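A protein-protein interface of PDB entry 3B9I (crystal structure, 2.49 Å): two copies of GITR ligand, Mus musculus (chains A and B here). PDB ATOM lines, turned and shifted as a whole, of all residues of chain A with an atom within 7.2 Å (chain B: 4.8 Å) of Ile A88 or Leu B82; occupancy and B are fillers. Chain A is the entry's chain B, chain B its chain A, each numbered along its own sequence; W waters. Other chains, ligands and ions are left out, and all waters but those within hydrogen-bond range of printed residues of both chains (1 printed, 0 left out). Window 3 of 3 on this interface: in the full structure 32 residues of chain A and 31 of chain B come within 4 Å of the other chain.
Of the 12 printed residues of chain A, 4 touch a printed residue of chain B. Hydrophobic or aromatic side chains of chain A that line the printed part of chain B: Ile A88 and Pro A90. Printed residues of chain B that touch a printed residue of chain A: Gln B80, Leu B82, Met B83, Pro B90 and Ile B91. Hydrophobic or aromatic side chains of chain B that line the printed part of chain A: Leu B82, Met B83 and Pro B90. Among the printed residues, no Asp or Glu carboxylate lies within 4 Å of a Lys or Arg side-chain nitrogen of the other chain.
The side-chain amide oxygen (OD1) of Asn A84 sits at hydrogen-bond distance from the backbone NH (N) of Gln A87 (2.7 Å). O of Val B70 sits at hydrogen-bond distance from N of Leu B82, at 2.7 Å. ND2 of Asn A84 lies within hydrogen-bond range of O of Ile A88 (3.2 Å).
Water W1 lies within hydrogen-bond range of the backbone carbonyl oxygen of Pro B90 (2.9 Å) and the backbone carbonyl oxygen of Pro A90 (3.0 Å).
The backbone carbonyl oxygen of Met B83 sits at hydrogen-bond distance from the side-chain amide nitrogen of Gln A87, at 3.4 Å.
Pro B90 touches its own counterpart, Pro A90. Of the 8 pairs that touch across the chains among the printed residues, 1 has its exchanged pair printed and touching as well.
Of chain B, only Gln B80 and Leu B82 come within 4 Å of Ile A88. Leu B82 touches two residues of chain A. Printed residues of chain A within 4 Å of Pro B90: Pro A90. Of the printed residues of chain B, Gln A53 touches Gln B80. Printed residues of chain A within 4 Å of Gln B80: Gln A53 (3.5 Å), Ile A88 (3.9 Å) and Pro A90 (3.7 Å). Of the printed residues of chain B, Gln A87 touches Met B83. Of the printed residues of chain A, Met B83 touches Gln A87 (3.4 Å). Asp A85 touches none of the printed residues of chain B. The nearest residue of chain A that does not touch Leu B82 is Gln A87 (5.2 Å). The nearest printed residue of chain B that does not touch Gln A53 is Ile B91 (6.6 Å).
Among the printed residues, pairs that only touch across the chains: Gln A53 with Gln B80 (3.5 Å), Pro A90 with Pro B90 (3.5 Å), Pro A90 with Leu B82 (3.6 Å), Pro A90 with Gln B80 (3.7 Å), Ile A88 with Gln B80 (3.9 Å), Pro A90 with Ile B91 (3.9 Å) and Ile A88 with Leu B82 (3.9 Å).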
ATOM      1  N   GLN A  53       0.564  -2.388  -1.863  1.00  0.00           N
ATOM      2  CA  GLN A  53       1.878  -2.910  -2.185  1.00  0.00           C
ATOM      3  C   GLN A  53       2.335  -2.230  -3.439  1.00  0.00           C
ATOM      4  O   GLN A  53       1.602  -2.180  -4.422  1.00  0.00           O
ATOM      5  CB  GLN A  53       1.849  -4.416  -2.372  1.00  0.00           C
ATOM      6  CG  GLN A  53       1.721  -5.194  -1.097  1.00  0.00           C
ATOM      7  CD  GLN A  53       1.755  -6.685  -1.364  1.00  0.00           C
ATOM      8  OE1 GLN A  53       1.922  -7.101  -2.503  1.00  0.00           O
ATOM      9  NE2 GLN A  53       1.606  -7.499  -0.314  1.00  0.00           N
ATOM     10  N   VAL A  54       3.536  -1.671  -3.409  1.00  0.00           N
ATOM     11  CA  VAL A  54       4.103  -1.090  -4.616  1.00  0.00           C
ATOM     12  C   VAL A  54       5.202  -1.996  -5.157  1.00  0.00           C
ATOM     13  O   VAL A  54       6.195  -2.245  -4.469  1.00  0.00           O
ATOM     14  CB  VAL A  54       4.623   0.284  -4.324  1.00  0.00           C
ATOM     15  CG1 VAL A  54       5.374   0.871  -5.558  1.00  0.00           C
ATOM     16  CG2 VAL A  54       3.455   1.161  -3.866  1.00  0.00           C
ATOM     17  N   ILE A  55       4.988  -2.519  -6.368  1.00  0.00           N
ATOM     18  CA  ILE A  55       5.903  -3.467  -7.000  1.00  0.00           C
ATOM     19  C   ILE A  55       6.820  -2.767  -8.007  1.00  0.00           C
ATOM     20  O   ILE A  55       6.352  -2.153  -8.975  1.00  0.00           O
ATOM     21  CB  ILE A  55       5.154  -4.586  -7.743  1.00  0.00           C
ATOM     22  CG1 ILE A  55       3.953  -5.106  -6.941  1.00  0.00           C
ATOM     23  CG2 ILE A  55       6.115  -5.719  -8.111  1.00  0.00           C
ATOM     24  CD1 ILE A  55       4.306  -6.008  -5.770  1.00  0.00           C
ATOM     25  N   PRO A  56       8.138  -2.842  -7.775  1.00  0.00           N
ATOM     26  CA  PRO A  56       9.055  -2.227  -8.717  1.00  0.00           C
ATOM     27  C   PRO A  56       9.334  -3.166  -9.874  1.00  0.00           C
ATOM     28  O   PRO A  56       9.283  -4.375  -9.710  1.00  0.00           O
ATOM     29  CB  PRO A  56      10.330  -2.066  -7.890  1.00  0.00           C
ATOM     30  CG  PRO A  56      10.298  -3.235  -6.974  1.00  0.00           C
ATOM     31  CD  PRO A  56       8.848  -3.461  -6.638  1.00  0.00           C
ATOM     32  N   PHE A  68      14.521   4.394  -5.888  1.00  0.00           N
ATOM     33  CA  PHE A  68      13.161   3.873  -5.693  1.00  0.00           C
ATOM     34  C   PHE A  68      12.574   4.428  -4.415  1.00  0.00           C
ATOM     35  O   PHE A  68      12.871   3.928  -3.337  1.00  0.00           O
ATOM     36  CB  PHE A  68      13.157   2.338  -5.645  1.00  0.00           C
ATOM     37  CG  PHE A  68      11.762   1.707  -5.539  1.00  0.00           C
ATOM     38  CD1 PHE A  68      10.755   2.033  -6.439  1.00  0.00           C
ATOM     39  CD2 PHE A  68      11.489   0.750  -4.564  1.00  0.00           C
ATOM     40  CE1 PHE A  68       9.496   1.452  -6.348  1.00  0.00           C
ATOM     41  CE2 PHE A  68      10.238   0.147  -4.474  1.00  0.00           C
ATOM     42  CZ  PHE A  68       9.234   0.499  -5.366  1.00  0.00           C
ATOM     43  N   ASN A  84      13.631   1.425  -0.889  1.00  0.00           N
ATOM     44  CA  ASN A  84      14.483   0.247  -0.765  1.00  0.00           C
ATOM     45  C   ASN A  84      15.245  -0.023  -2.059  1.00  0.00           C
ATOM     46  O   ASN A  84      15.172   0.756  -3.001  1.00  0.00           O
ATOM     47  CB  ASN A  84      13.694  -0.986  -0.284  1.00  0.00           C
ATOM     48  CG  ASN A  84      12.666  -1.472  -1.302  1.00  0.00           C
ATOM     49  OD1 ASN A  84      12.843  -1.302  -2.499  1.00  0.00           O
ATOM     50  ND2 ASN A  84      11.599  -2.102  -0.820  1.00  0.00           N
ATOM     51  N   ASP A  85      15.979  -1.125  -2.108  1.00  0.00           N
ATOM     52  CA  ASP A  85      16.765  -1.419  -3.291  1.00  0.00           C
ATOM     53  C   ASP A  85      15.890  -2.086  -4.353  1.00  0.00           C
ATOM     54  O   ASP A  85      16.106  -3.245  -4.685  1.00  0.00           O
ATOM     55  CB  ASP A  85      17.954  -2.305  -2.923  1.00  0.00           C
ATOM     56  CG  ASP A  85      19.026  -2.301  -3.986  1.00  0.00           C
ATOM     57  OD1 ASP A  85      19.053  -1.359  -4.812  1.00  0.00           O
ATOM     58  OD2 ASP A  85      19.836  -3.253  -3.997  1.00  0.00           O
ATOM     59  N   PHE A  86      14.903  -1.341  -4.858  1.00  0.00           N
ATOM     60  CA  PHE A  86      13.905  -1.820  -5.835  1.00  0.00           C
ATOM     61  C   PHE A  86      13.269  -3.171  -5.545  1.00  0.00           C
ATOM     62  O   PHE A  86      13.295  -4.062  -6.393  1.00  0.00           O
ATOM     63  CB  PHE A  86      14.486  -1.816  -7.243  1.00  0.00           C
ATOM     64  CG  PHE A  86      14.854  -0.457  -7.709  1.00  0.00           C
ATOM     65  CD1 PHE A  86      14.001   0.255  -8.512  1.00  0.00           C
ATOM     66  CD2 PHE A  86      16.045   0.137  -7.286  1.00  0.00           C
ATOM     67  CE1 PHE A  86      14.326   1.520  -8.919  1.00  0.00           C
ATOM     68  CE2 PHE A  86      16.378   1.406  -7.693  1.00  0.00           C
ATOM     69  CZ  PHE A  86      15.519   2.103  -8.509  1.00  0.00           C
ATOM     70  N   GLN A  87      12.705  -3.316  -4.351  1.00  0.00           N
ATOM     71  CA  GLN A  87      12.048  -4.551  -3.950  1.00  0.00           C
ATOM     72  C   GLN A  87      10.586  -4.282  -3.623  1.00  0.00           C
ATOM     73  O   GLN A  87      10.159  -3.126  -3.562  1.00  0.00           O
ATOM     74  CB  GLN A  87      12.728  -5.130  -2.717  1.00  0.00           C
ATOM     75  CG  GLN A  87      14.183  -5.410  -2.888  1.00  0.00           C
ATOM     76  CD  GLN A  87      14.861  -5.722  -1.564  1.00  0.00           C
ATOM     77  OE1 GLN A  87      16.056  -6.009  -1.537  1.00  0.00           O
ATOM     78  NE2 GLN A  87      14.108  -5.668  -0.464  1.00  0.00           N
ATOM     79  N   ILE A  88       9.830  -5.351  -3.391  1.00  0.00           N
ATOM     80  CA  ILE A  88       8.428  -5.235  -3.022  1.00  0.00           C
ATOM     81  C   ILE A  88       8.298  -4.246  -1.867  1.00  0.00           C
ATOM     82  O   ILE A  88       9.138  -4.212  -0.974  1.00  0.00           O
ATOM     83  CB  ILE A  88       7.832  -6.614  -2.651  1.00  0.00           C
ATOM     84  CG1 ILE A  88       6.366  -6.485  -2.230  1.00  0.00           C
ATOM     85  CG2 ILE A  88       8.693  -7.330  -1.579  1.00  0.00           C
ATOM     86  CD1 ILE A  88       5.771  -7.779  -1.648  1.00  0.00           C
ATOM     87  N   LEU A  89       7.261  -3.420  -1.902  1.00  0.00           N
ATOM     88  CA  LEU A  89       7.128  -2.400  -0.898  1.00  0.00           C
ATOM     89  C   LEU A  89       5.710  -2.294  -0.380  1.00  0.00           C
ATOM     90  O   LEU A  89       4.888  -1.566  -0.948  1.00  0.00           O
ATOM     91  CB  LEU A  89       7.569  -1.062  -1.478  1.00  0.00           C
ATOM     92  CG  LEU A  89       7.877   0.076  -0.521  1.00  0.00           C
ATOM     93  CD1 LEU A  89       8.903  -0.342   0.542  1.00  0.00           C
ATOM     94  CD2 LEU A  89       8.450   1.202  -1.359  1.00  0.00           C
ATOM     95  N   PRO A  90       5.396  -3.044   0.677  1.00  0.00           N
ATOM     96  CA  PRO A  90       4.127  -2.766   1.375  1.00  0.00           C
ATOM     97  C   PRO A  90       4.171  -1.363   1.948  1.00  0.00           C
ATOM     98  O   PRO A  90       5.227  -0.918   2.389  1.00  0.00           O
ATOM     99  CB  PRO A  90       4.090  -3.786   2.515  1.00  0.00           C
ATOM    100  CG  PRO A  90       5.172  -4.790   2.213  1.00  0.00           C
ATOM    101  CD  PRO A  90       6.133  -4.189   1.227  1.00  0.00           C
ATOM    102  N   PHE B  68      18.602  -6.377   8.505  1.00  0.00           N
ATOM    103  CA  PHE B  68      17.286  -6.245   9.090  1.00  0.00           C
ATOM    104  C   PHE B  68      16.275  -6.917   8.151  1.00  0.00           C
ATOM    105  O   PHE B  68      15.938  -6.354   7.120  1.00  0.00           O
ATOM    106  CB  PHE B  68      16.972  -4.755   9.232  1.00  0.00           C
ATOM    107  CG  PHE B  68      15.584  -4.458   9.740  1.00  0.00           C
ATOM    108  CD1 PHE B  68      15.098  -5.067  10.893  1.00  0.00           C
ATOM    109  CD2 PHE B  68      14.777  -3.545   9.082  1.00  0.00           C
ATOM    110  CE1 PHE B  68      13.819  -4.791  11.356  1.00  0.00           C
ATOM    111  CE2 PHE B  68      13.505  -3.245   9.560  1.00  0.00           C
ATOM    112  CZ  PHE B  68      13.022  -3.866  10.690  1.00  0.00           C
ATOM    113  N   VAL B  69      15.797  -8.111   8.502  1.00  0.00           N
ATOM    114  CA  VAL B  69      14.851  -8.836   7.652  1.00  0.00           C
ATOM    115  C   VAL B  69      13.609  -9.285   8.422  1.00  0.00           C
ATOM    116  O   VAL B  69      13.700  -9.764   9.554  1.00  0.00           O
ATOM    117  CB  VAL B  69      15.500 -10.077   6.961  1.00  0.00           C
ATOM    118  CG1 VAL B  69      14.524 -10.742   5.976  1.00  0.00           C
ATOM    119  CG2 VAL B  69      16.790  -9.692   6.241  1.00  0.00           C
ATOM    120  N   VAL B  70      12.451  -9.126   7.786  1.00  0.00           N
ATOM    121  CA  VAL B  70      11.177  -9.559   8.345  1.00  0.00           C
ATOM    122  C   VAL B  70      10.455 -10.434   7.318  1.00  0.00           C
ATOM    123  O   VAL B  70      10.339 -10.056   6.143  1.00  0.00           O
ATOM    124  CB  VAL B  70      10.284  -8.341   8.672  1.00  0.00           C
ATOM    125  CG1 VAL B  70       8.861  -8.777   9.068  1.00  0.00           C
ATOM    126  CG2 VAL B  70      10.923  -7.496   9.759  1.00  0.00           C
ATOM    127  N   GLN B  80       5.811 -13.243   2.390  1.00  0.00           N
ATOM    128  CA  GLN B  80       6.665 -12.180   1.877  1.00  0.00           C
ATOM    129  C   GLN B  80       7.895 -12.005   2.739  1.00  0.00           C
ATOM    130  O   GLN B  80       7.861 -12.250   3.941  1.00  0.00           O
ATOM    131  CB  GLN B  80       5.922 -10.832   1.764  1.00  0.00           C
ATOM    132  CG  GLN B  80       5.273 -10.312   3.041  1.00  0.00           C
ATOM    133  CD  GLN B  80       4.798  -8.870   2.936  1.00  0.00           C
ATOM    134  OE1 GLN B  80       4.962  -8.092   3.864  1.00  0.00           O
ATOM    135  NE2 GLN B  80       4.196  -8.513   1.811  1.00  0.00           N
ATOM    136  N   THR B  81       8.969 -11.544   2.108  1.00  0.00           N
ATOM    137  CA  THR B  81      10.234 -11.315   2.768  1.00  0.00           C
ATOM    138  C   THR B  81      10.541  -9.851   2.560  1.00  0.00           C
ATOM    139  O   THR B  81      10.528  -9.391   1.441  1.00  0.00           O
ATOM    140  CB  THR B  81      11.340 -12.187   2.118  1.00  0.00           C
ATOM    141  OG1 THR B  81      10.997 -13.568   2.271  1.00  0.00           O
ATOM    142  CG2 THR B  81      12.724 -11.927   2.737  1.00  0.00           C
ATOM    143  N   LEU B  82      10.807  -9.113   3.632  1.00  0.00           N
ATOM    144  CA  LEU B  82      11.132  -7.694   3.504  1.00  0.00           C
ATOM    145  C   LEU B  82      12.454  -7.345   4.188  1.00  0.00           C
ATOM    146  O   LEU B  82      12.800  -7.910   5.251  1.00  0.00           O
ATOM    147  CB  LEU B  82      10.012  -6.842   4.094  1.00  0.00           C
ATOM    148  CG  LEU B  82       8.557  -7.173   3.767  1.00  0.00           C
ATOM    149  CD1 LEU B  82       7.655  -6.363   4.687  1.00  0.00           C
ATOM    150  CD2 LEU B  82       8.254  -6.895   2.305  1.00  0.00           C
ATOM    151  N   MET B  83      13.195  -6.428   3.571  1.00  0.00           N
ATOM    152  CA  MET B  83      14.447  -5.916   4.125  1.00  0.00           C
ATOM    153  C   MET B  83      14.632  -4.463   3.721  1.00  0.00           C
ATOM    154  O   MET B  83      14.445  -4.096   2.561  1.00  0.00           O
ATOM    155  CB  MET B  83      15.683  -6.775   3.730  1.00  0.00           C
ATOM    156  CG  MET B  83      15.647  -7.384   2.319  1.00  0.00           C
ATOM    157  SD  MET B  83      16.668  -8.879   1.984  1.00  0.00           S
ATOM    158  CE  MET B  83      15.685  -9.750   0.723  1.00  0.00           C
ATOM    159  N   ASN B  84      14.951  -3.623   4.698  1.00  0.00           N
ATOM    160  CA  ASN B  84      15.514  -2.311   4.414  1.00  0.00           C
ATOM    161  C   ASN B  84      16.677  -2.046   5.376  1.00  0.00           C
ATOM    162  O   ASN B  84      17.009  -2.882   6.214  1.00  0.00           O
ATOM    163  CB  ASN B  84      14.455  -1.201   4.422  1.00  0.00           C
ATOM    164  CG  ASN B  84      13.878  -0.931   5.807  1.00  0.00           C
ATOM    165  OD1 ASN B  84      14.466  -1.282   6.834  1.00  0.00           O
ATOM    166  ND2 ASN B  84      12.727  -0.279   5.840  1.00  0.00           N
ATOM    167  N   LEU B  89       9.385  -0.266   8.987  1.00  0.00           N
ATOM    168  CA  LEU B  89       8.970  -1.187   7.940  1.00  0.00           C
ATOM    169  C   LEU B  89       7.494  -1.534   8.064  1.00  0.00           C
ATOM    170  O   LEU B  89       7.109  -2.254   8.984  1.00  0.00           O
ATOM    171  CB  LEU B  89       9.816  -2.453   8.042  1.00  0.00           C
ATOM    172  CG  LEU B  89       9.716  -3.511   6.959  1.00  0.00           C
ATOM    173  CD1 LEU B  89      10.228  -2.925   5.642  1.00  0.00           C
ATOM    174  CD2 LEU B  89      10.554  -4.710   7.366  1.00  0.00           C
ATOM    175  N   PRO B  90       6.644  -0.966   7.184  1.00  0.00           N
ATOM    176  CA  PRO B  90       5.275  -1.459   7.024  1.00  0.00           C
ATOM    177  C   PRO B  90       5.264  -2.818   6.310  1.00  0.00           C
ATOM    178  O   PRO B  90       6.042  -3.045   5.375  1.00  0.00           O
ATOM    179  CB  PRO B  90       4.609  -0.391   6.139  1.00  0.00           C
ATOM    180  CG  PRO B  90       5.527   0.784   6.169  1.00  0.00           C
ATOM    181  CD  PRO B  90       6.899   0.213   6.338  1.00  0.00           C
ATOM    182  N   ILE B  91       4.370  -3.697   6.747  1.00  0.00           N
ATOM    183  CA  ILE B  91       4.343  -5.070   6.285  1.00  0.00           C
ATOM    184  C   ILE B  91       2.940  -5.449   5.832  1.00  0.00           C
ATOM    185  O   ILE B  91       1.969  -4.814   6.226  1.00  0.00           O
ATOM    186  CB  ILE B  91       4.755  -6.063   7.424  1.00  0.00           C
ATOM    187  CG1 ILE B  91       3.677  -6.133   8.514  1.00  0.00           C
ATOM    188  CG2 ILE B  91       6.102  -5.684   8.026  1.00  0.00           C
ATOM    189  CD1 ILE B  91       3.940  -7.200   9.609  1.00  0.00           C
HETATM  190  O   HOH W   1       7.880  -1.919   3.427  1.00  0.00           O
